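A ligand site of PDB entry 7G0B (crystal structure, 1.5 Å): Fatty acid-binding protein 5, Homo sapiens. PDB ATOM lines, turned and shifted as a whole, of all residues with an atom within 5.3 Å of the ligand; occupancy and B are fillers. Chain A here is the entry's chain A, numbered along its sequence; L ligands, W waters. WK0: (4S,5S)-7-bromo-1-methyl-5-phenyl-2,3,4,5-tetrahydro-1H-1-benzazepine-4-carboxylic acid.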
ATOM      1  N   LEU A  16     -18.461  24.174   7.314  1.00  0.00           N
ATOM      2  CA  LEU A  16     -17.281  24.962   7.732  1.00  0.00           C
ATOM      3  C   LEU A  16     -16.234  24.994   6.586  1.00  0.00           C
ATOM      4  O   LEU A  16     -15.783  23.921   6.155  1.00  0.00           O
ATOM      5  CB  LEU A  16     -16.612  24.378   8.927  1.00  0.00           C
ATOM      6  CG  LEU A  16     -15.398  25.191   9.439  1.00  0.00           C
ATOM      7  CD1 LEU A  16     -15.835  26.567  10.033  1.00  0.00           C
ATOM      8  CD2 LEU A  16     -14.613  24.365  10.449  1.00  0.00           C
ATOM      9  N   PHE A  22      -9.827  29.904  16.559  1.00  0.00           N
ATOM     10  CA  PHE A  22     -10.618  28.961  17.351  1.00  0.00           C
ATOM     11  C   PHE A  22      -9.843  28.328  18.503  1.00  0.00           C
ATOM     12  O   PHE A  22     -10.376  28.220  19.629  1.00  0.00           O
ATOM     13  CB  PHE A  22     -11.335  27.926  16.421  1.00  0.00           C
ATOM     14  CG  PHE A  22     -12.353  27.065  17.147  1.00  0.00           C
ATOM     15  CD1 PHE A  22     -13.325  27.645  17.991  1.00  0.00           C
ATOM     16  CD2 PHE A  22     -12.330  25.723  16.970  1.00  0.00           C
ATOM     17  CE1 PHE A  22     -14.261  26.817  18.652  1.00  0.00           C
ATOM     18  CE2 PHE A  22     -13.266  24.895  17.648  1.00  0.00           C
ATOM     19  CZ  PHE A  22     -14.180  25.457  18.454  1.00  0.00           C
ATOM     20  N   TYR A  25      -9.575  30.923  21.267  1.00  0.00           N
ATOM     21  CA  TYR A  25     -10.870  31.080  21.933  1.00  0.00           C
ATOM     22  C   TYR A  25     -11.139  29.906  22.868  1.00  0.00           C
ATOM     23  O   TYR A  25     -11.525  30.090  24.029  1.00  0.00           O
ATOM     24  CB  TYR A  25     -11.963  31.214  20.902  1.00  0.00           C
ATOM     25  CG  TYR A  25     -13.366  31.267  21.492  1.00  0.00           C
ATOM     26  CD1 TYR A  25     -13.820  32.362  22.224  1.00  0.00           C
ATOM     27  CD2 TYR A  25     -14.277  30.229  21.305  1.00  0.00           C
ATOM     28  CE1 TYR A  25     -15.046  32.364  22.757  1.00  0.00           C
ATOM     29  CE2 TYR A  25     -15.520  30.286  21.792  1.00  0.00           C
ATOM     30  CZ  TYR A  25     -15.914  31.341  22.561  1.00  0.00           C
ATOM     31  OH  TYR A  25     -17.208  31.387  23.080  1.00  0.00           O
ATOM     32  N   MET A  26     -10.858  28.682  22.427  1.00  0.00           N
ATOM     33  CA  MET A  26     -11.012  27.527  23.351  1.00  0.00           C
ATOM     34  C   MET A  26     -10.096  27.573  24.574  1.00  0.00           C
ATOM     35  O   MET A  26     -10.525  27.241  25.683  1.00  0.00           O
ATOM     36  CB  MET A  26     -10.836  26.184  22.579  1.00  0.00           C
ATOM     37  CG  MET A  26     -11.978  25.933  21.636  1.00  0.00           C
ATOM     38  SD  MET A  26     -11.845  24.225  20.982  1.00  0.00           S
ATOM     39  CE  MET A  26     -10.488  24.394  19.857  1.00  0.00           C
ATOM     40  N   LEU A  29     -11.611  29.968  27.063  1.00  0.00           N
ATOM     41  CA  LEU A  29     -12.720  29.250  27.742  1.00  0.00           C
ATOM     42  C   LEU A  29     -12.150  28.233  28.785  1.00  0.00           C
ATOM     43  O   LEU A  29     -12.908  27.785  29.669  1.00  0.00           O
ATOM     44  CB  LEU A  29     -13.593  28.502  26.772  1.00  0.00           C
ATOM     45  CG  LEU A  29     -14.540  29.236  25.805  1.00  0.00           C
ATOM     46  CD1 LEU A  29     -15.197  28.273  24.845  1.00  0.00           C
ATOM     47  CD2 LEU A  29     -15.574  30.095  26.572  1.00  0.00           C
ATOM     48  N   VAL A  31     -10.784  25.244  27.908  1.00  0.00           N
ATOM     49  CA  VAL A  31     -11.143  23.895  27.374  1.00  0.00           C
ATOM     50  C   VAL A  31      -9.893  23.069  27.432  1.00  0.00           C
ATOM     51  O   VAL A  31      -8.809  23.528  27.064  1.00  0.00           O
ATOM     52  CB  VAL A  31     -11.683  23.987  25.966  1.00  0.00           C
ATOM     53  CG1 VAL A  31     -12.004  22.626  25.347  1.00  0.00           C
ATOM     54  CG2 VAL A  31     -12.985  24.786  25.934  1.00  0.00           C
ATOM     55  N   LEU A  35     -10.835  18.037  24.226  1.00  0.00           N
ATOM     56  CA  LEU A  35     -11.783  18.827  23.503  1.00  0.00           C
ATOM     57  C   LEU A  35     -11.165  19.816  22.491  1.00  0.00           C
ATOM     58  O   LEU A  35     -11.699  20.040  21.405  1.00  0.00           O
ATOM     59  CB  LEU A  35     -12.740  19.543  24.495  1.00  0.00           C
ATOM     60  CG  LEU A  35     -13.760  18.640  25.232  1.00  0.00           C
ATOM     61  CD1 LEU A  35     -14.278  19.201  26.580  1.00  0.00           C
ATOM     62  CD2 LEU A  35     -14.951  18.260  24.290  1.00  0.00           C
ATOM     63  N   GLY A  39     -11.944  19.870  18.530  1.00  0.00           N
ATOM     64  CA  GLY A  39     -12.255  21.142  17.855  1.00  0.00           C
ATOM     65  C   GLY A  39     -11.302  21.492  16.741  1.00  0.00           C
ATOM     66  O   GLY A  39     -11.717  22.024  15.711  1.00  0.00           O
ATOM     67  N   ALA A  42     -12.594  18.573  13.887  1.00  0.00           N
ATOM     68  CA  ALA A  42     -13.974  18.470  13.388  1.00  0.00           C
ATOM     69  C   ALA A  42     -14.141  19.513  12.230  1.00  0.00           C
ATOM     70  O   ALA A  42     -13.591  20.611  12.287  1.00  0.00           O
ATOM     71  CB  ALA A  42     -14.990  18.669  14.558  1.00  0.00           C
ATOM     72  N   PRO A  44     -17.355  20.720  11.092  1.00  0.00           N
ATOM     73  CA  PRO A  44     -18.816  20.521  11.247  1.00  0.00           C
ATOM     74  C   PRO A  44     -19.650  21.202  10.215  1.00  0.00           C
ATOM     75  O   PRO A  44     -19.230  22.104   9.447  1.00  0.00           O
ATOM     76  CB  PRO A  44     -19.091  21.128  12.600  1.00  0.00           C
ATOM     77  CG  PRO A  44     -18.027  22.190  12.713  1.00  0.00           C
ATOM     78  CD  PRO A  44     -16.855  21.507  12.221  1.00  0.00           C
ATOM     79  N   THR A  59     -24.976  21.679  15.592  1.00  0.00           N
ATOM     80  CA  THR A  59     -23.673  21.725  14.977  1.00  0.00           C
ATOM     81  C   THR A  59     -23.228  20.259  14.930  1.00  0.00           C
ATOM     82  O   THR A  59     -23.128  19.595  15.909  1.00  0.00           O
ATOM     83  CB  THR A  59     -22.737  22.633  15.780  1.00  0.00           C
ATOM     84  OG1 THR A  59     -23.387  23.905  15.947  1.00  0.00           O
ATOM     85  CG2 THR A  59     -21.435  22.838  15.006  1.00  0.00           C
ATOM     86  N   SER A  61     -20.943  16.982  13.420  1.00  0.00           N
ATOM     87  CA  SER A  61     -19.741  16.354  12.764  1.00  0.00           C
ATOM     88  C   SER A  61     -19.564  14.957  13.309  1.00  0.00           C
ATOM     89  O   SER A  61     -20.145  14.609  14.306  1.00  0.00           O
ATOM     90  CB  SER A  61     -18.501  17.205  13.029  1.00  0.00           C
ATOM     91  OG  SER A  61     -18.108  17.091  14.373  1.00  0.00           O
ATOM     92  N   LYS A  64     -18.044  15.350  16.779  1.00  0.00           N
ATOM     93  CA  LYS A  64     -18.874  15.924  17.808  1.00  0.00           C
ATOM     94  C   LYS A  64     -20.095  16.621  17.240  1.00  0.00           C
ATOM     95  O   LYS A  64     -19.998  17.387  16.254  1.00  0.00           O
ATOM     96  CB  LYS A  64     -18.115  16.900  18.709  1.00  0.00           C
ATOM     97  CG  LYS A  64     -18.823  17.052  20.076  1.00  0.00           C
ATOM     98  CD  LYS A  64     -18.255  18.152  20.943  1.00  0.00           C
ATOM     99  CE  LYS A  64     -18.588  17.917  22.421  1.00  0.00           C
ATOM    100  NZ  LYS A  64     -20.059  17.744  22.686  1.00  0.00           N
ATOM    101  N   THR A  66     -23.579  18.893  18.725  1.00  0.00           N
ATOM    102  CA  THR A  66     -24.301  19.588  19.819  1.00  0.00           C
ATOM    103  C   THR A  66     -25.574  20.161  19.206  1.00  0.00           C
ATOM    104  O   THR A  66     -25.684  20.406  17.998  1.00  0.00           O
ATOM    105  CB  THR A  66     -23.485  20.736  20.391  1.00  0.00           C
ATOM    106  OG1 THR A  66     -23.355  21.742  19.371  1.00  0.00           O
ATOM    107  CG2 THR A  66     -22.101  20.244  20.814  1.00  0.00           C
ATOM    108  N   ALA A  81     -20.730  22.870  24.012  1.00  0.00           N
ATOM    109  CA  ALA A  81     -19.911  21.741  23.520  1.00  0.00           C
ATOM    110  C   ALA A  81     -18.874  21.252  24.483  1.00  0.00           C
ATOM    111  O   ALA A  81     -18.592  20.052  24.546  1.00  0.00           O
ATOM    112  CB  ALA A  81     -19.237  22.113  22.174  1.00  0.00           C
ATOM    113  N   ASP A  82     -18.266  22.189  25.204  1.00  0.00           N
ATOM    114  CA  ASP A  82     -17.289  21.932  26.164  1.00  0.00           C
ATOM    115  C   ASP A  82     -17.793  21.632  27.582  1.00  0.00           C
ATOM    116  O   ASP A  82     -17.019  21.397  28.500  1.00  0.00           O
ATOM    117  CB  ASP A  82     -16.251  23.092  26.151  1.00  0.00           C
ATOM    118  CG  ASP A  82     -16.888  24.466  26.453  1.00  0.00           C
ATOM    119  OD1 ASP A  82     -17.802  24.907  25.736  1.00  0.00           O
ATOM    120  OD2 ASP A  82     -16.358  25.029  27.452  1.00  0.00           O
ATOM    121  N   ARG A  84     -19.909  23.476  29.601  1.00  0.00           N
ATOM    122  CA  ARG A  84     -20.407  24.557  30.505  1.00  0.00           C
ATOM    123  C   ARG A  84     -21.932  24.546  30.557  1.00  0.00           C
ATOM    124  O   ARG A  84     -22.611  24.185  29.590  1.00  0.00           O
ATOM    125  CB  ARG A  84     -19.915  25.926  30.062  1.00  0.00           C
ATOM    126  CG  ARG A  84     -18.439  26.143  30.238  1.00  0.00           C
ATOM    127  CD  ARG A  84     -18.021  27.418  29.576  1.00  0.00           C
ATOM    128  NE  ARG A  84     -17.983  27.269  28.124  1.00  0.00           N
ATOM    129  CZ  ARG A  84     -18.577  28.036  27.208  1.00  0.00           C
ATOM    130  NH1 ARG A  84     -19.162  29.175  27.542  1.00  0.00           N
ATOM    131  NH2 ARG A  84     -18.562  27.676  25.924  1.00  0.00           N
ATOM    132  N   GLN A 101     -23.810  34.354  26.386  1.00  0.00           N
ATOM    133  CA  GLN A 101     -23.664  33.347  27.435  1.00  0.00           C
ATOM    134  C   GLN A 101     -23.072  33.934  28.691  1.00  0.00           C
ATOM    135  O   GLN A 101     -22.039  34.621  28.621  1.00  0.00           O
ATOM    136  CB  GLN A 101     -22.740  32.225  26.965  1.00  0.00           C
ATOM    137  CG  GLN A 101     -23.164  31.494  25.765  1.00  0.00           C
ATOM    138  CD  GLN A 101     -22.113  30.501  25.303  1.00  0.00           C
ATOM    139  OE1 GLN A 101     -20.882  30.654  25.501  1.00  0.00           O
ATOM    140  NE2 GLN A 101     -22.596  29.454  24.683  1.00  0.00           N
ATOM    141  N   ILE A 110     -21.428  34.923  20.897  1.00  0.00           N
ATOM    142  CA  ILE A 110     -21.269  34.279  19.584  1.00  0.00           C
ATOM    143  C   ILE A 110     -22.228  34.960  18.662  1.00  0.00           C
ATOM    144  O   ILE A 110     -23.444  34.983  18.976  1.00  0.00           O
ATOM    145  CB  ILE A 110     -21.614  32.818  19.620  1.00  0.00           C
ATOM    146  CG1 ILE A 110     -20.701  32.105  20.597  1.00  0.00           C
ATOM    147  CG2 ILE A 110     -21.477  32.219  18.192  1.00  0.00           C
ATOM    148  CD1 ILE A 110     -21.283  30.817  21.078  1.00  0.00           C
ATOM    149  N   ARG A 112     -23.761  35.284  14.571  1.00  0.00           N
ATOM    150  CA  ARG A 112     -23.890  34.603  13.297  1.00  0.00           C
ATOM    151  C   ARG A 112     -24.600  35.564  12.334  1.00  0.00           C
ATOM    152  O   ARG A 112     -25.664  36.088  12.601  1.00  0.00           O
ATOM    153  CB  ARG A 112     -24.657  33.305  13.458  1.00  0.00           C
ATOM    154  CG  ARG A 112     -23.962  32.312  14.426  1.00  0.00           C
ATOM    155  CD  ARG A 112     -24.704  30.987  14.478  1.00  0.00           C
ATOM    156  NE  ARG A 112     -24.032  29.990  15.294  1.00  0.00           N
ATOM    157  CZ  ARG A 112     -24.161  29.917  16.640  1.00  0.00           C
ATOM    158  NH1 ARG A 112     -24.857  30.775  17.299  1.00  0.00           N
ATOM    159  NH2 ARG A 112     -23.582  28.912  17.290  1.00  0.00           N
ATOM    160  N   VAL A 121     -19.506  33.147  11.542  1.00  0.00           N
ATOM    161  CA  VAL A 121     -19.669  32.889  12.987  1.00  0.00           C
ATOM    162  C   VAL A 121     -18.461  33.468  13.725  1.00  0.00           C
ATOM    163  O   VAL A 121     -17.365  33.057  13.485  1.00  0.00           O
ATOM    164  CB  VAL A 121     -19.769  31.395  13.252  1.00  0.00           C
ATOM    165  CG1 VAL A 121     -19.976  31.138  14.747  1.00  0.00           C
ATOM    166  CG2 VAL A 121     -20.989  30.810  12.450  1.00  0.00           C
ATOM    167  N   CYS A 123     -16.867  34.394  17.544  1.00  0.00           N
ATOM    168  CA  CYS A 123     -16.909  34.143  18.994  1.00  0.00           C
ATOM    169  C   CYS A 123     -15.995  35.104  19.710  1.00  0.00           C
ATOM    170  O   CYS A 123     -14.979  35.479  19.194  1.00  0.00           O
ATOM    171  CB  CYS A 123     -16.467  32.723  19.249  1.00  0.00           C
ATOM    172  SG  CYS A 123     -17.566  31.499  18.426  1.00  0.00           S
ATOM    173  N   ARG A 132     -15.225  31.983  12.089  1.00  0.00           N
ATOM    174  CA  ARG A 132     -15.479  30.719  11.336  1.00  0.00           C
ATOM    175  C   ARG A 132     -16.476  30.997  10.225  1.00  0.00           C
ATOM    176  O   ARG A 132     -17.511  31.592  10.385  1.00  0.00           O
ATOM    177  CB  ARG A 132     -15.935  29.591  12.247  1.00  0.00           C
ATOM    178  CG  ARG A 132     -14.764  29.188  13.137  1.00  0.00           C
ATOM    179  CD  ARG A 132     -15.166  28.439  14.330  1.00  0.00           C
ATOM    180  NE  ARG A 132     -15.659  27.092  14.143  1.00  0.00           N
ATOM    181  CZ  ARG A 132     -14.919  25.986  14.036  1.00  0.00           C
ATOM    182  NH1 ARG A 132     -13.634  26.023  13.853  1.00  0.00           N
ATOM    183  NH2 ARG A 132     -15.524  24.812  14.021  1.00  0.00           N
ATOM    184  N   TYR A 134     -18.719  29.592   7.005  1.00  0.00           N
ATOM    185  CA  TYR A 134     -19.474  28.451   6.522  1.00  0.00           C
ATOM    186  C   TYR A 134     -20.125  28.813   5.179  1.00  0.00           C
ATOM    187  O   TYR A 134     -20.583  29.922   4.963  1.00  0.00           O
ATOM    188  CB  TYR A 134     -20.551  28.109   7.528  1.00  0.00           C
ATOM    189  CG  TYR A 134     -20.123  27.520   8.886  1.00  0.00           C
ATOM    190  CD1 TYR A 134     -19.564  28.304   9.966  1.00  0.00           C
ATOM    191  CD2 TYR A 134     -20.319  26.191   9.099  1.00  0.00           C
ATOM    192  CE1 TYR A 134     -19.269  27.614  11.178  1.00  0.00           C
ATOM    193  CE2 TYR A 134     -20.009  25.532  10.324  1.00  0.00           C
ATOM    194  CZ  TYR A 134     -19.485  26.276  11.320  1.00  0.00           C
ATOM    195  OH  TYR A 134     -19.233  25.555  12.501  1.00  0.00           O
HETATM  196  C1  WK0 L   1     -17.881  26.101  16.984  1.00  0.00           C
HETATM  197  C2  WK0 L   1     -18.423  25.088  18.021  1.00  0.00           C
HETATM  198  C3  WK0 L   1     -18.253  23.623  17.605  1.00  0.00           C
HETATM  199  C4  WK0 L   1     -17.041  23.223  16.965  1.00  0.00           C
HETATM  200  C5  WK0 L   1     -16.901  21.877  16.545  1.00  0.00           C
HETATM  201  C6  WK0 L   1     -17.931  20.953  16.801  1.00  0.00           C
HETATM  202  C7  WK0 L   1     -19.103  21.334  17.471  1.00  0.00           C
HETATM  203  C8  WK0 L   1     -19.243  22.663  17.885  1.00  0.00           C
HETATM  204  C9  WK0 L   1     -20.219  28.165  20.345  1.00  0.00           C
HETATM  205  C10 WK0 L   1     -18.988  28.101  18.233  1.00  0.00           C
HETATM  206  C11 WK0 L   1     -18.728  26.163  15.748  1.00  0.00           C
HETATM  207  C12 WK0 L   1     -17.930  25.337  19.428  1.00  0.00           C
HETATM  208  C13 WK0 L   1     -18.380  26.506  20.127  1.00  0.00           C
HETATM  209  N14 WK0 L   1     -19.301  27.342  19.494  1.00  0.00           N
HETATM  210  O15 WK0 L   1     -19.995  26.286  15.865  1.00  0.00           O
HETATM  211  O16 WK0 L   1     -18.152  26.118  14.598  1.00  0.00           O
HETATM  212  C17 WK0 L   1     -17.728  27.511  17.586  1.00  0.00           C
HETATM  213  C18 WK0 L   1     -17.094  25.821  22.045  1.00  0.00           C
HETATM  214  C19 WK0 L   1     -17.971  26.728  21.467  1.00  0.00           C
HETATM  215  C20 WK0 L   1     -17.060  24.451  20.036  1.00  0.00           C
HETATM  216  C21 WK0 L   1     -16.621  24.688  21.348  1.00  0.00           C
HETATM  217 BR22 WK0 L   1     -15.365  23.380  22.090  1.00  0.00          BR
HETATM  218  O   HOH W   1     -22.246  27.969  14.390  1.00  0.00           O
HETATM  219  O   HOH W   2     -22.315  27.423  22.456  1.00  0.00           O
HETATM  220  O   HOH W   3     -21.582  23.937  19.860  1.00  0.00           O
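O16 of the ligand sits at hydrogen-bond distance from OH of Tyr 134. The guanidinium group of Arg 132 lies within salt-bridge range of an oxygen (O16) of the ligand, 2.7 Å away.
N of Arg 132 is in hydrogen-bond range of O of Val 121 (2.8 Å). N of Thr 59 lies within hydrogen-bond range of O of Thr 66 (2.8 Å). NZ of Lys 64 lies close to O of Ala 81 (3.3 Å). The backbone carbonyl oxygen (O) of Met 26 lies within hydrogen-bond range of the backbone NH (N) of Val 31. NE of Arg 84 is in salt-bridge range of OD2 of Asp 82, at 2.8 Å.
CZ of Phe 22 touches C20 of the ligand (3.4 Å). Met 26 touches the ligand. Thr 59 touches the ligand (CG2 to C8, 3.6 Å). Ala 81 touches the ligand. Asp 82 touches the ligand (OD1 to C18, 3.9 Å). Ile 110 touches the ligand. SG of Cys 123 touches C10 of the ligand, at 3.7 Å. Of the 24 residues printed, 9 come within 4 Å of the ligand.
Water W1 lies within hydrogen-bond range of the guanidinium group of Arg 112 (2.8 Å) and an oxygen (O15) of the ligand (3.2 Å).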
